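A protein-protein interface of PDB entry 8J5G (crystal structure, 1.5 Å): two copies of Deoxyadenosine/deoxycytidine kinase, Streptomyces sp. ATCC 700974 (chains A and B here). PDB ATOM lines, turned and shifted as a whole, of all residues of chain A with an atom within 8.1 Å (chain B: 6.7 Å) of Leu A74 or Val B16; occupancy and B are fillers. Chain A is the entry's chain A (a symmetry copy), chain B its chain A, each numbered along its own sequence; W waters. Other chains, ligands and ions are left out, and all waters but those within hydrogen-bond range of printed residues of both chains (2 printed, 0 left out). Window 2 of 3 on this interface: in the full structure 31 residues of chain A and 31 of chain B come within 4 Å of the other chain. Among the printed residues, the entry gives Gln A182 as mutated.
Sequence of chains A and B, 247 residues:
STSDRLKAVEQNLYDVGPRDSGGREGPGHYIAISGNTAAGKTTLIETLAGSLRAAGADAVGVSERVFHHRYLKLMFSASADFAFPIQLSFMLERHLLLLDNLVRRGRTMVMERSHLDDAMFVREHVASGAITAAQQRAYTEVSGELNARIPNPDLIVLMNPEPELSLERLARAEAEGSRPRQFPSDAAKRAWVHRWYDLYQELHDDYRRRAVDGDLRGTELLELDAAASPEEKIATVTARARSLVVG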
ATOM      1  N   HIS A  69      -5.265  27.445 -33.992  1.00  0.00           N
ATOM      2  CA  HIS A  69      -6.271  26.479 -34.393  1.00  0.00           C
ATOM      3  C   HIS A  69      -7.324  26.309 -33.303  1.00  0.00           C
ATOM      4  O   HIS A  69      -7.040  26.449 -32.110  1.00  0.00           O
ATOM      5  CB  HIS A  69      -5.610  25.132 -34.686  1.00  0.00           C
ATOM      6  CG  HIS A  69      -6.421  24.257 -35.577  1.00  0.00           C
ATOM      7  ND1 HIS A  69      -7.478  23.504 -35.114  1.00  0.00           N
ATOM      8  CD2 HIS A  69      -6.353  24.036 -36.908  1.00  0.00           C
ATOM      9  CE1 HIS A  69      -8.022  22.850 -36.123  1.00  0.00           C
ATOM     10  NE2 HIS A  69      -7.371  23.174 -37.230  1.00  0.00           N
ATOM     11  N   ARG A  70      -8.550  25.977 -33.723  1.00  0.00           N
ATOM     12  CA  ARG A  70      -9.572  25.586 -32.751  1.00  0.00           C
ATOM     13  C   ARG A  70      -9.101  24.477 -31.819  1.00  0.00           C
ATOM     14  O   ARG A  70      -9.533  24.422 -30.665  1.00  0.00           O
ATOM     15  CB  ARG A  70     -10.857  25.163 -33.471  1.00  0.00           C
ATOM     16  CG  ARG A  70     -11.711  26.344 -33.936  1.00  0.00           C
ATOM     17  CD  ARG A  70     -12.713  25.969 -35.021  1.00  0.00           C
ATOM     18  NE  ARG A  70     -12.028  25.570 -36.244  1.00  0.00           N
ATOM     19  CZ  ARG A  70     -12.621  25.339 -37.408  1.00  0.00           C
ATOM     20  NH1 ARG A  70     -13.927  25.486 -37.560  1.00  0.00           N
ATOM     21  NH2 ARG A  70     -11.882  24.961 -38.447  1.00  0.00           N
ATOM     22  N   TYR A  71      -8.208  23.603 -32.283  1.00  0.00           N
ATOM     23  CA  TYR A  71      -7.708  22.494 -31.487  1.00  0.00           C
ATOM     24  C   TYR A  71      -6.413  22.814 -30.737  1.00  0.00           C
ATOM     25  O   TYR A  71      -5.782  21.886 -30.222  1.00  0.00           O
ATOM     26  CB  TYR A  71      -7.467  21.284 -32.391  1.00  0.00           C
ATOM     27  CG  TYR A  71      -8.686  20.544 -32.879  1.00  0.00           C
ATOM     28  CD1 TYR A  71      -9.728  20.203 -32.013  1.00  0.00           C
ATOM     29  CD2 TYR A  71      -8.758  20.103 -34.193  1.00  0.00           C
ATOM     30  CE1 TYR A  71     -10.822  19.482 -32.467  1.00  0.00           C
ATOM     31  CE2 TYR A  71      -9.848  19.386 -34.657  1.00  0.00           C
ATOM     32  CZ  TYR A  71     -10.868  19.076 -33.788  1.00  0.00           C
ATOM     33  OH  TYR A  71     -11.944  18.348 -34.240  1.00  0.00           O
ATOM     34  N   LEU A  72      -6.012  24.093 -30.670  1.00  0.00           N
ATOM     35  CA  LEU A  72      -4.719  24.469 -30.095  1.00  0.00           C
ATOM     36  C   LEU A  72      -4.469  23.810 -28.740  1.00  0.00           C
ATOM     37  O   LEU A  72      -3.374  23.296 -28.482  1.00  0.00           O
ATOM     38  CB  LEU A  72      -4.633  25.993 -29.962  1.00  0.00           C
ATOM     39  CG  LEU A  72      -3.366  26.546 -29.300  1.00  0.00           C
ATOM     40  CD1 LEU A  72      -2.135  26.151 -30.095  1.00  0.00           C
ATOM     41  CD2 LEU A  72      -3.467  28.046 -29.195  1.00  0.00           C
ATOM     42  N   LYS A  73      -5.470  23.830 -27.853  1.00  0.00           N
ATOM     43  CA  LYS A  73      -5.257  23.321 -26.496  1.00  0.00           C
ATOM     44  C   LYS A  73      -4.864  21.850 -26.485  1.00  0.00           C
ATOM     45  O   LYS A  73      -4.174  21.408 -25.554  1.00  0.00           O
ATOM     46  CB  LYS A  73      -6.499  23.543 -25.627  1.00  0.00           C
ATOM     47  CG  LYS A  73      -6.695  25.008 -25.173  1.00  0.00           C
ATOM     48  CD  LYS A  73      -7.926  25.114 -24.278  1.00  0.00           C
ATOM     49  CE  LYS A  73      -8.179  26.521 -23.786  1.00  0.00           C
ATOM     50  NZ  LYS A  73      -9.328  26.522 -22.830  1.00  0.00           N
ATOM     51  N   LEU A  74      -5.265  21.082 -27.505  1.00  0.00           N
ATOM     52  CA  LEU A  74      -4.901  19.670 -27.542  1.00  0.00           C
ATOM     53  C   LEU A  74      -3.410  19.465 -27.811  1.00  0.00           C
ATOM     54  O   LEU A  74      -2.869  18.427 -27.424  1.00  0.00           O
ATOM     55  CB  LEU A  74      -5.753  18.916 -28.576  1.00  0.00           C
ATOM     56  CG  LEU A  74      -7.237  18.742 -28.212  1.00  0.00           C
ATOM     57  CD1 LEU A  74      -8.033  18.167 -29.397  1.00  0.00           C
ATOM     58  CD2 LEU A  74      -7.438  17.857 -26.982  1.00  0.00           C
ATOM     59  N   MET A  75      -2.730  20.427 -28.450  1.00  0.00           N
ATOM     60  CA  MET A  75      -1.274  20.357 -28.560  1.00  0.00           C
ATOM     61  C   MET A  75      -0.635  20.222 -27.177  1.00  0.00           C
ATOM     62  O   MET A  75       0.425  19.609 -27.024  1.00  0.00           O
ATOM     63  CB  MET A  75      -0.733  21.659 -29.147  1.00  0.00           C
ATOM     64  CG  MET A  75       0.788  21.756 -29.316  1.00  0.00           C
ATOM     65  SD  MET A  75       1.484  22.246 -30.905  1.00  0.00           S
ATOM     66  CE  MET A  75       1.043  23.976 -30.667  1.00  0.00           C
ATOM     67  N   PHE A  76      -1.216  20.889 -26.174  1.00  0.00           N
ATOM     68  CA  PHE A  76      -0.615  20.970 -24.845  1.00  0.00           C
ATOM     69  C   PHE A  76      -1.223  20.007 -23.839  1.00  0.00           C
ATOM     70  O   PHE A  76      -0.570  19.708 -22.845  1.00  0.00           O
ATOM     71  CB  PHE A  76      -0.709  22.411 -24.332  1.00  0.00           C
ATOM     72  CG  PHE A  76      -0.018  23.379 -25.219  1.00  0.00           C
ATOM     73  CD1 PHE A  76       1.353  23.332 -25.370  1.00  0.00           C
ATOM     74  CD2 PHE A  76      -0.744  24.289 -25.951  1.00  0.00           C
ATOM     75  CE1 PHE A  76       2.005  24.212 -26.224  1.00  0.00           C
ATOM     76  CE2 PHE A  76      -0.094  25.171 -26.805  1.00  0.00           C
ATOM     77  CZ  PHE A  76       1.280  25.131 -26.927  1.00  0.00           C
ATOM     78  N   SER A  77      -2.437  19.508 -24.076  1.00  0.00           N
ATOM     79  CA  SER A  77      -3.016  18.494 -23.200  1.00  0.00           C
ATOM     80  C   SER A  77      -2.831  17.075 -23.703  1.00  0.00           C
ATOM     81  O   SER A  77      -2.970  16.137 -22.909  1.00  0.00           O
ATOM     82  CB  SER A  77      -4.514  18.752 -22.993  1.00  0.00           C
ATOM     83  OG  SER A  77      -5.229  18.592 -24.214  1.00  0.00           O
ATOM     84  N   ALA A  78      -2.567  16.881 -24.996  1.00  0.00           N
ATOM     85  CA  ALA A  78      -2.389  15.560 -25.592  1.00  0.00           C
ATOM     86  C   ALA A  78      -1.291  15.662 -26.649  1.00  0.00           C
ATOM     87  O   ALA A  78      -1.491  15.399 -27.836  1.00  0.00           O
ATOM     88  CB  ALA A  78      -3.695  15.044 -26.192  1.00  0.00           C
ATOM     89  N   SER A  79      -0.095  16.048 -26.200  1.00  0.00           N
ATOM     90  CA  SER A  79       0.922  16.503 -27.146  1.00  0.00           C
ATOM     91  C   SER A  79       1.425  15.386 -28.051  1.00  0.00           C
ATOM     92  O   SER A  79       1.786  15.647 -29.203  1.00  0.00           O
ATOM     93  CB  SER A  79       2.096  17.144 -26.400  1.00  0.00           C
ATOM     94  OG  SER A  79       2.719  16.200 -25.539  1.00  0.00           O
ATOM     95  N   ALA A  80       1.477  14.147 -27.565  1.00  0.00           N
ATOM     96  CA  ALA A  80       2.010  13.102 -28.427  1.00  0.00           C
ATOM     97  C   ALA A  80       1.046  12.720 -29.533  1.00  0.00           C
ATOM     98  O   ALA A  80       1.445  11.999 -30.450  1.00  0.00           O
ATOM     99  CB  ALA A  80       2.388  11.862 -27.615  1.00  0.00           C
ATOM    100  N   ASP A  81      -0.198  13.192 -29.472  1.00  0.00           N
ATOM    101  CA  ASP A  81      -1.175  13.024 -30.539  1.00  0.00           C
ATOM    102  C   ASP A  81      -1.329  14.269 -31.403  1.00  0.00           C
ATOM    103  O   ASP A  81      -1.449  14.158 -32.626  1.00  0.00           O
ATOM    104  CB  ASP A  81      -2.530  12.645 -29.938  1.00  0.00           C
ATOM    105  CG  ASP A  81      -2.473  11.336 -29.174  1.00  0.00           C
ATOM    106  OD1 ASP A  81      -2.048  10.332 -29.782  1.00  0.00           O
ATOM    107  OD2 ASP A  81      -2.830  11.324 -27.976  1.00  0.00           O
ATOM    108  N   PHE A  82      -1.304  15.462 -30.807  1.00  0.00           N
ATOM    109  CA  PHE A  82      -1.702  16.663 -31.536  1.00  0.00           C
ATOM    110  C   PHE A  82      -0.578  17.657 -31.815  1.00  0.00           C
ATOM    111  O   PHE A  82      -0.787  18.583 -32.604  1.00  0.00           O
ATOM    112  CB  PHE A  82      -2.853  17.361 -30.789  1.00  0.00           C
ATOM    113  CG  PHE A  82      -4.177  16.663 -30.975  1.00  0.00           C
ATOM    114  CD1 PHE A  82      -4.549  15.596 -30.165  1.00  0.00           C
ATOM    115  CD2 PHE A  82      -5.010  17.013 -32.029  1.00  0.00           C
ATOM    116  CE1 PHE A  82      -5.748  14.935 -30.365  1.00  0.00           C
ATOM    117  CE2 PHE A  82      -6.205  16.352 -32.245  1.00  0.00           C
ATOM    118  CZ  PHE A  82      -6.577  15.304 -31.407  1.00  0.00           C
ATOM    119  N   ALA A  83       0.608  17.498 -31.225  1.00  0.00           N
ATOM    120  CA  ALA A  83       1.678  18.461 -31.493  1.00  0.00           C
ATOM    121  C   ALA A  83       2.104  18.449 -32.957  1.00  0.00           C
ATOM    122  O   ALA A  83       2.316  19.515 -33.543  1.00  0.00           O
ATOM    123  CB  ALA A  83       2.880  18.189 -30.587  1.00  0.00           C
ATOM    124  N   PHE A  84       2.231  17.261 -33.573  1.00  0.00           N
ATOM    125  CA  PHE A  84       2.650  17.213 -34.977  1.00  0.00           C
ATOM    126  C   PHE A  84       1.647  17.914 -35.883  1.00  0.00           C
ATOM    127  O   PHE A  84       2.038  18.868 -36.582  1.00  0.00           O
ATOM    128  CB  PHE A  84       2.914  15.757 -35.386  1.00  0.00           C
ATOM    129  CG  PHE A  84       3.309  15.566 -36.837  1.00  0.00           C
ATOM    130  CD1 PHE A  84       4.415  16.218 -37.387  1.00  0.00           C
ATOM    131  CD2 PHE A  84       2.584  14.684 -37.641  1.00  0.00           C
ATOM    132  CE1 PHE A  84       4.768  16.002 -38.728  1.00  0.00           C
ATOM    133  CE2 PHE A  84       2.932  14.456 -38.969  1.00  0.00           C
ATOM    134  CZ  PHE A  84       4.027  15.119 -39.514  1.00  0.00           C
ATOM    135  N   ILE A  86      -0.795  20.085 -35.177  1.00  0.00           N
ATOM    136  CA  ILE A  86      -0.974  21.504 -34.859  1.00  0.00           C
ATOM    137  C   ILE A  86       0.259  22.317 -35.251  1.00  0.00           C
ATOM    138  O   ILE A  86       0.136  23.466 -35.702  1.00  0.00           O
ATOM    139  CB  ILE A  86      -1.350  21.699 -33.379  1.00  0.00           C
ATOM    140  CG1 ILE A  86      -2.700  21.052 -33.088  1.00  0.00           C
ATOM    141  CG2 ILE A  86      -1.376  23.205 -33.038  1.00  0.00           C
ATOM    142  CD1 ILE A  86      -3.878  21.729 -33.751  1.00  0.00           C
ATOM    143  N   HIS A 125       9.146  19.834 -29.270  1.00  0.00           N
ATOM    144  CA  HIS A 125       8.340  18.626 -29.113  1.00  0.00           C
ATOM    145  C   HIS A 125       9.135  17.369 -29.459  1.00  0.00           C
ATOM    146  O   HIS A 125       8.842  16.289 -28.928  1.00  0.00           O
ATOM    147  CB  HIS A 125       7.085  18.690 -29.988  1.00  0.00           C
ATOM    148  CG  HIS A 125       6.037  19.645 -29.507  1.00  0.00           C
ATOM    149  ND1 HIS A 125       5.323  19.444 -28.344  1.00  0.00           N
ATOM    150  CD2 HIS A 125       5.556  20.787 -30.053  1.00  0.00           C
ATOM    151  CE1 HIS A 125       4.457  20.432 -28.188  1.00  0.00           C
ATOM    152  NE2 HIS A 125       4.572  21.258 -29.218  1.00  0.00           N
ATOM    153  N   ARG A 181      -6.815  30.146 -21.061  1.00  0.00           N
ATOM    154  CA  ARG A 181      -5.829  29.255 -20.433  1.00  0.00           C
ATOM    155  C   ARG A 181      -5.486  28.110 -21.374  1.00  0.00           C
ATOM    156  O   ARG A 181      -6.227  27.129 -21.483  1.00  0.00           O
ATOM    157  CB  ARG A 181      -6.334  28.694 -19.108  1.00  0.00           C
ATOM    158  CG  ARG A 181      -6.293  29.653 -17.958  1.00  0.00           C
ATOM    159  CD  ARG A 181      -6.504  28.938 -16.624  1.00  0.00           C
ATOM    160  NE  ARG A 181      -6.705  29.919 -15.567  1.00  0.00           N
ATOM    161  CZ  ARG A 181      -5.729  30.596 -14.976  1.00  0.00           C
ATOM    162  NH1 ARG A 181      -4.455  30.337 -15.227  1.00  0.00           N
ATOM    163  NH2 ARG A 181      -6.039  31.561 -14.111  1.00  0.00           N
ATOM    164  N   GLN A 182      -4.331  28.207 -22.032  1.00  0.00           N
ATOM    165  CA  GLN A 182      -3.990  27.263 -23.090  1.00  0.00           C
ATOM    166  C   GLN A 182      -3.402  25.954 -22.574  1.00  0.00           C
ATOM    167  O   GLN A 182      -3.396  24.966 -23.313  1.00  0.00           O
ATOM    168  CB  GLN A 182      -3.003  27.908 -24.069  1.00  0.00           C
ATOM    169  CG  GLN A 182      -3.414  29.293 -24.575  1.00  0.00           C
ATOM    170  CD  GLN A 182      -4.514  29.264 -25.632  1.00  0.00           C
ATOM    171  OE1 GLN A 182      -5.292  28.307 -25.732  1.00  0.00           O
ATOM    172  NE2 GLN A 182      -4.580  30.323 -26.432  1.00  0.00           N
ATOM    173  N   PRO A 184      -2.696  22.607 -19.712  1.00  0.00           N
ATOM    174  CA  PRO A 184      -3.498  21.731 -18.838  1.00  0.00           C
ATOM    175  C   PRO A 184      -3.218  21.898 -17.357  1.00  0.00           C
ATOM    176  O   PRO A 184      -3.928  21.294 -16.534  1.00  0.00           O
ATOM    177  CB  PRO A 184      -3.092  20.325 -19.297  1.00  0.00           C
ATOM    178  CG  PRO A 184      -1.696  20.486 -19.834  1.00  0.00           C
ATOM    179  CD  PRO A 184      -1.709  21.843 -20.501  1.00  0.00           C
ATOM    180  N   TRP A 192       6.648  24.799 -20.436  1.00  0.00           N
ATOM    181  CA  TRP A 192       6.753  25.159 -21.856  1.00  0.00           C
ATOM    182  C   TRP A 192       7.384  26.533 -22.022  1.00  0.00           C
ATOM    183  O   TRP A 192       8.236  26.727 -22.898  1.00  0.00           O
ATOM    184  CB  TRP A 192       5.382  25.099 -22.547  1.00  0.00           C
ATOM    185  CG  TRP A 192       5.205  23.859 -23.426  1.00  0.00           C
ATOM    186  CD1 TRP A 192       5.912  23.553 -24.560  1.00  0.00           C
ATOM    187  CD2 TRP A 192       4.273  22.773 -23.233  1.00  0.00           C
ATOM    188  NE1 TRP A 192       5.485  22.361 -25.090  1.00  0.00           N
ATOM    189  CE2 TRP A 192       4.480  21.855 -24.297  1.00  0.00           C
ATOM    190  CE3 TRP A 192       3.277  22.493 -22.278  1.00  0.00           C
ATOM    191  CZ2 TRP A 192       3.735  20.681 -24.427  1.00  0.00           C
ATOM    192  CZ3 TRP A 192       2.536  21.329 -22.414  1.00  0.00           C
ATOM    193  CH2 TRP A 192       2.766  20.439 -23.483  1.00  0.00           C
ATOM    194  N   ASN B  12     -20.789  19.681 -32.238  1.00  0.00           N
ATOM    195  CA  ASN B  12     -19.671  19.689 -31.291  1.00  0.00           C
ATOM    196  C   ASN B  12     -18.389  19.135 -31.914  1.00  0.00           C
ATOM    197  O   ASN B  12     -17.701  18.302 -31.322  1.00  0.00           O
ATOM    198  CB  ASN B  12     -20.024  18.911 -30.021  1.00  0.00           C
ATOM    199  CG  ASN B  12     -19.149  19.296 -28.844  1.00  0.00           C
ATOM    200  OD1 ASN B  12     -18.559  20.379 -28.824  1.00  0.00           O
ATOM    201  ND2 ASN B  12     -19.017  18.389 -27.881  1.00  0.00           N
ATOM    202  N   TYR B  14     -15.520  20.644 -32.580  1.00  0.00           N
ATOM    203  CA  TYR B  14     -14.250  21.186 -32.085  1.00  0.00           C
ATOM    204  C   TYR B  14     -14.216  21.348 -30.571  1.00  0.00           C
ATOM    205  O   TYR B  14     -13.931  22.433 -30.053  1.00  0.00           O
ATOM    206  CB  TYR B  14     -13.940  22.522 -32.766  1.00  0.00           C
ATOM    207  CG  TYR B  14     -13.904  22.430 -34.254  1.00  0.00           C
ATOM    208  CD1 TYR B  14     -12.785  21.924 -34.903  1.00  0.00           C
ATOM    209  CD2 TYR B  14     -15.008  22.779 -35.018  1.00  0.00           C
ATOM    210  CE1 TYR B  14     -12.750  21.817 -36.291  1.00  0.00           C
ATOM    211  CE2 TYR B  14     -14.990  22.666 -36.384  1.00  0.00           C
ATOM    212  CZ  TYR B  14     -13.869  22.182 -37.021  1.00  0.00           C
ATOM    213  OH  TYR B  14     -13.870  22.089 -38.392  1.00  0.00           O
ATOM    214  N   ASP B  15     -14.453  20.260 -29.863  1.00  0.00           N
ATOM    215  CA  ASP B  15     -14.465  20.237 -28.407  1.00  0.00           C
ATOM    216  C   ASP B  15     -13.114  19.714 -27.935  1.00  0.00           C
ATOM    217  O   ASP B  15     -12.759  18.567 -28.227  1.00  0.00           O
ATOM    218  CB  ASP B  15     -15.614  19.344 -27.923  1.00  0.00           C
ATOM    219  CG  ASP B  15     -15.795  19.340 -26.407  1.00  0.00           C
ATOM    220  OD1 ASP B  15     -14.983  19.930 -25.664  1.00  0.00           O
ATOM    221  OD2 ASP B  15     -16.780  18.713 -25.953  1.00  0.00           O
ATOM    222  N   VAL B  16     -12.356  20.544 -27.214  1.00  0.00           N
ATOM    223  CA  VAL B  16     -11.044  20.106 -26.741  1.00  0.00           C
ATOM    224  C   VAL B  16     -11.145  19.531 -25.328  1.00  0.00           C
ATOM    225  O   VAL B  16     -10.128  19.186 -24.716  1.00  0.00           O
ATOM    226  CB  VAL B  16     -10.013  21.251 -26.796  1.00  0.00           C
ATOM    227  CG1 VAL B  16      -9.839  21.736 -28.231  1.00  0.00           C
ATOM    228  CG2 VAL B  16     -10.434  22.395 -25.893  1.00  0.00           C
ATOM    229  N   GLY B  17     -12.369  19.392 -24.816  1.00  0.00           N
ATOM    230  CA  GLY B  17     -12.577  18.806 -23.511  1.00  0.00           C
ATOM    231  C   GLY B  17     -12.420  17.301 -23.528  1.00  0.00           C
ATOM    232  O   GLY B  17     -12.148  16.677 -24.560  1.00  0.00           O
ATOM    233  N   PRO B  18     -12.605  16.691 -22.359  1.00  0.00           N
ATOM    234  CA  PRO B  18     -12.318  15.256 -22.220  1.00  0.00           C
ATOM    235  C   PRO B  18     -13.330  14.357 -22.914  1.00  0.00           C
ATOM    236  O   PRO B  18     -14.497  14.707 -23.104  1.00  0.00           O
ATOM    237  CB  PRO B  18     -12.335  15.023 -20.702  1.00  0.00           C
ATOM    238  CG  PRO B  18     -12.925  16.232 -20.096  1.00  0.00           C
ATOM    239  CD  PRO B  18     -13.025  17.329 -21.102  1.00  0.00           C
ATOM    240  N   LEU B  96      -7.048  16.350 -38.537  1.00  0.00           N
ATOM    241  CA  LEU B  96      -7.287  16.847 -37.181  1.00  0.00           C
ATOM    242  C   LEU B  96      -8.709  16.546 -36.729  1.00  0.00           C
ATOM    243  O   LEU B  96      -8.933  16.100 -35.593  1.00  0.00           O
ATOM    244  CB  LEU B  96      -7.020  18.352 -37.127  1.00  0.00           C
ATOM    245  CG  LEU B  96      -5.556  18.740 -37.021  1.00  0.00           C
ATOM    246  CD1 LEU B  96      -5.419  20.212 -37.383  1.00  0.00           C
ATOM    247  CD2 LEU B  96      -5.067  18.467 -35.598  1.00  0.00           C
ATOM    248  N   ASP B 100      -9.398  13.983 -33.546  1.00  0.00           N
ATOM    249  CA  ASP B 100     -10.144  14.398 -32.362  1.00  0.00           C
ATOM    250  C   ASP B 100     -11.463  13.638 -32.221  1.00  0.00           C
ATOM    251  O   ASP B 100     -11.736  13.051 -31.168  1.00  0.00           O
ATOM    252  CB  ASP B 100     -10.419  15.901 -32.402  1.00  0.00           C
ATOM    253  CG  ASP B 100     -11.457  16.317 -31.377  1.00  0.00           C
ATOM    254  OD1 ASP B 100     -11.226  16.071 -30.175  1.00  0.00           O
ATOM    255  OD2 ASP B 100     -12.505  16.871 -31.769  1.00  0.00           O
ATOM    256  N   ARG B 104      -9.770  10.260 -30.627  1.00  0.00           N
ATOM    257  CA  ARG B 104      -9.688  10.723 -29.241  1.00  0.00           C
ATOM    258  C   ARG B 104     -11.034  10.616 -28.527  1.00  0.00           C
ATOM    259  O   ARG B 104     -11.113  10.120 -27.393  1.00  0.00           O
ATOM    260  CB  ARG B 104      -9.177  12.162 -29.207  1.00  0.00           C
ATOM    261  CG  ARG B 104      -8.954  12.699 -27.794  1.00  0.00           C
ATOM    262  CD  ARG B 104      -8.497  14.153 -27.824  1.00  0.00           C
ATOM    263  NE  ARG B 104      -9.606  15.082 -27.997  1.00  0.00           N
ATOM    264  CZ  ARG B 104     -10.336  15.572 -27.005  1.00  0.00           C
ATOM    265  NH1 ARG B 104     -10.159  15.177 -25.751  1.00  0.00           N
ATOM    266  NH2 ARG B 104     -11.268  16.480 -27.275  1.00  0.00           N
ATOM    267  N   ARG B 105     -12.110  11.080 -29.162  1.00  0.00           N
ATOM    268  CA  ARG B 105     -13.403  11.121 -28.482  1.00  0.00           C
ATOM    269  C   ARG B 105     -14.307   9.943 -28.816  1.00  0.00           C
ATOM    270  O   ARG B 105     -15.408   9.845 -28.255  1.00  0.00           O
ATOM    271  CB  ARG B 105     -14.118  12.439 -28.788  1.00  0.00           C
ATOM    272  CG  ARG B 105     -13.415  13.631 -28.104  1.00  0.00           C
ATOM    273  CD  ARG B 105     -14.324  14.831 -28.042  1.00  0.00           C
ATOM    274  NE  ARG B 105     -14.247  15.603 -29.273  1.00  0.00           N
ATOM    275  CZ  ARG B 105     -15.252  16.265 -29.828  1.00  0.00           C
ATOM    276  NH1 ARG B 105     -16.485  16.190 -29.351  1.00  0.00           N
ATOM    277  NH2 ARG B 105     -15.006  17.052 -30.869  1.00  0.00           N
HETATM  278  O   HOH W   1      -7.423  20.247 -24.234  1.00  0.00           O
HETATM  279  O   HOH W   2     -12.003  24.722 -29.677  1.00  0.00           O
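Water W2 bridges the backbone carbonyl oxygen of Arg A70 (2.7 Å) and the backbone carbonyl oxygen of Tyr B14 (3.0 Å). Water W1 lies within hydrogen-bond range of the side-chain hydroxyl (OG) of Ser A77 and the backbone carbonyl oxygen (O) of Val B16.
No position is printed for both chains.
Leu B96 touches His A69 (CD1 to NE2, 3.6 Å). CD1 of Tyr B14 touches CZ of Tyr A71, 3.6 Å away. Leu B96 touches Tyr A71 (O to CE2, 3.5 Å). O of Val B16 touches CD2 of Leu A74, at 3.8 Å. Asp B100 touches Leu A74 (OD1 to CD1, 3.9 Å). CD2 of Leu A74 touches NE of Arg B104, 3.7 Å away. Leu B96 touches Phe A82. N of Asp B100 touches CZ of Phe A82, at 3.8 Å. CE1 of Phe A82 touches CD of Arg B104, 3.8 Å away. Ile A86 touches Leu B96 (CD1 to CD2, 3.9 Å).
Hydrophobic or aromatic side chains of chain B within 4 Å of the printed part of chain A: Tyr B14, Val B16 and Leu B96. Among the printed residues, 14 pairs touch across the chains.
OD1 of Asp B100 is in salt-bridge range of NE of Arg B104. A ring nitrogen (ND1) of His A69 is in hydrogen-bond range of the backbone NH (N) of Tyr A71, at 2.9 Å. The backbone carbonyl oxygen (O) of Gly B17 lies within hydrogen-bond range of the guanidinium group (NH1) of Arg B104, 2.8 Å away. The side-chain carboxylate (OD2) of Asp B100 is in salt-bridge range of the guanidinium group (NH2) of Arg B105, at 2.7 Å. O of Asp B15 sits at hydrogen-bond distance from NH2 of Arg B104 (2.7 Å).
Of the printed residues of chain B, Tyr A71 touches Tyr B14 (3.6 Å), Val B16 (3.96 Å), Leu B96 (3.5 Å) and Asp B100 (2.9 Å). Leu A74 touches just these residues of chain B: Val B16, Asp B100 and Arg B104. Asp A81 touches none of the printed residues of chain B. Of the printed residues of chain B, Ile A86 touches Leu B96 (3.9 Å). Val B16 touches just these residues of chain A: Arg A70, Tyr A71 and Leu A74. The nearest residue of chain B that does not touch Leu A74 is Asp B15 (4.9 Å).
The side-chain carboxylate of Asp B100 is in hydrogen-bond range of the side-chain hydroxyl of Tyr A71 (2.9 Å). The guanidinium group of Arg A70 lies within hydrogen-bond range of the side-chain hydroxyl of Tyr B14.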
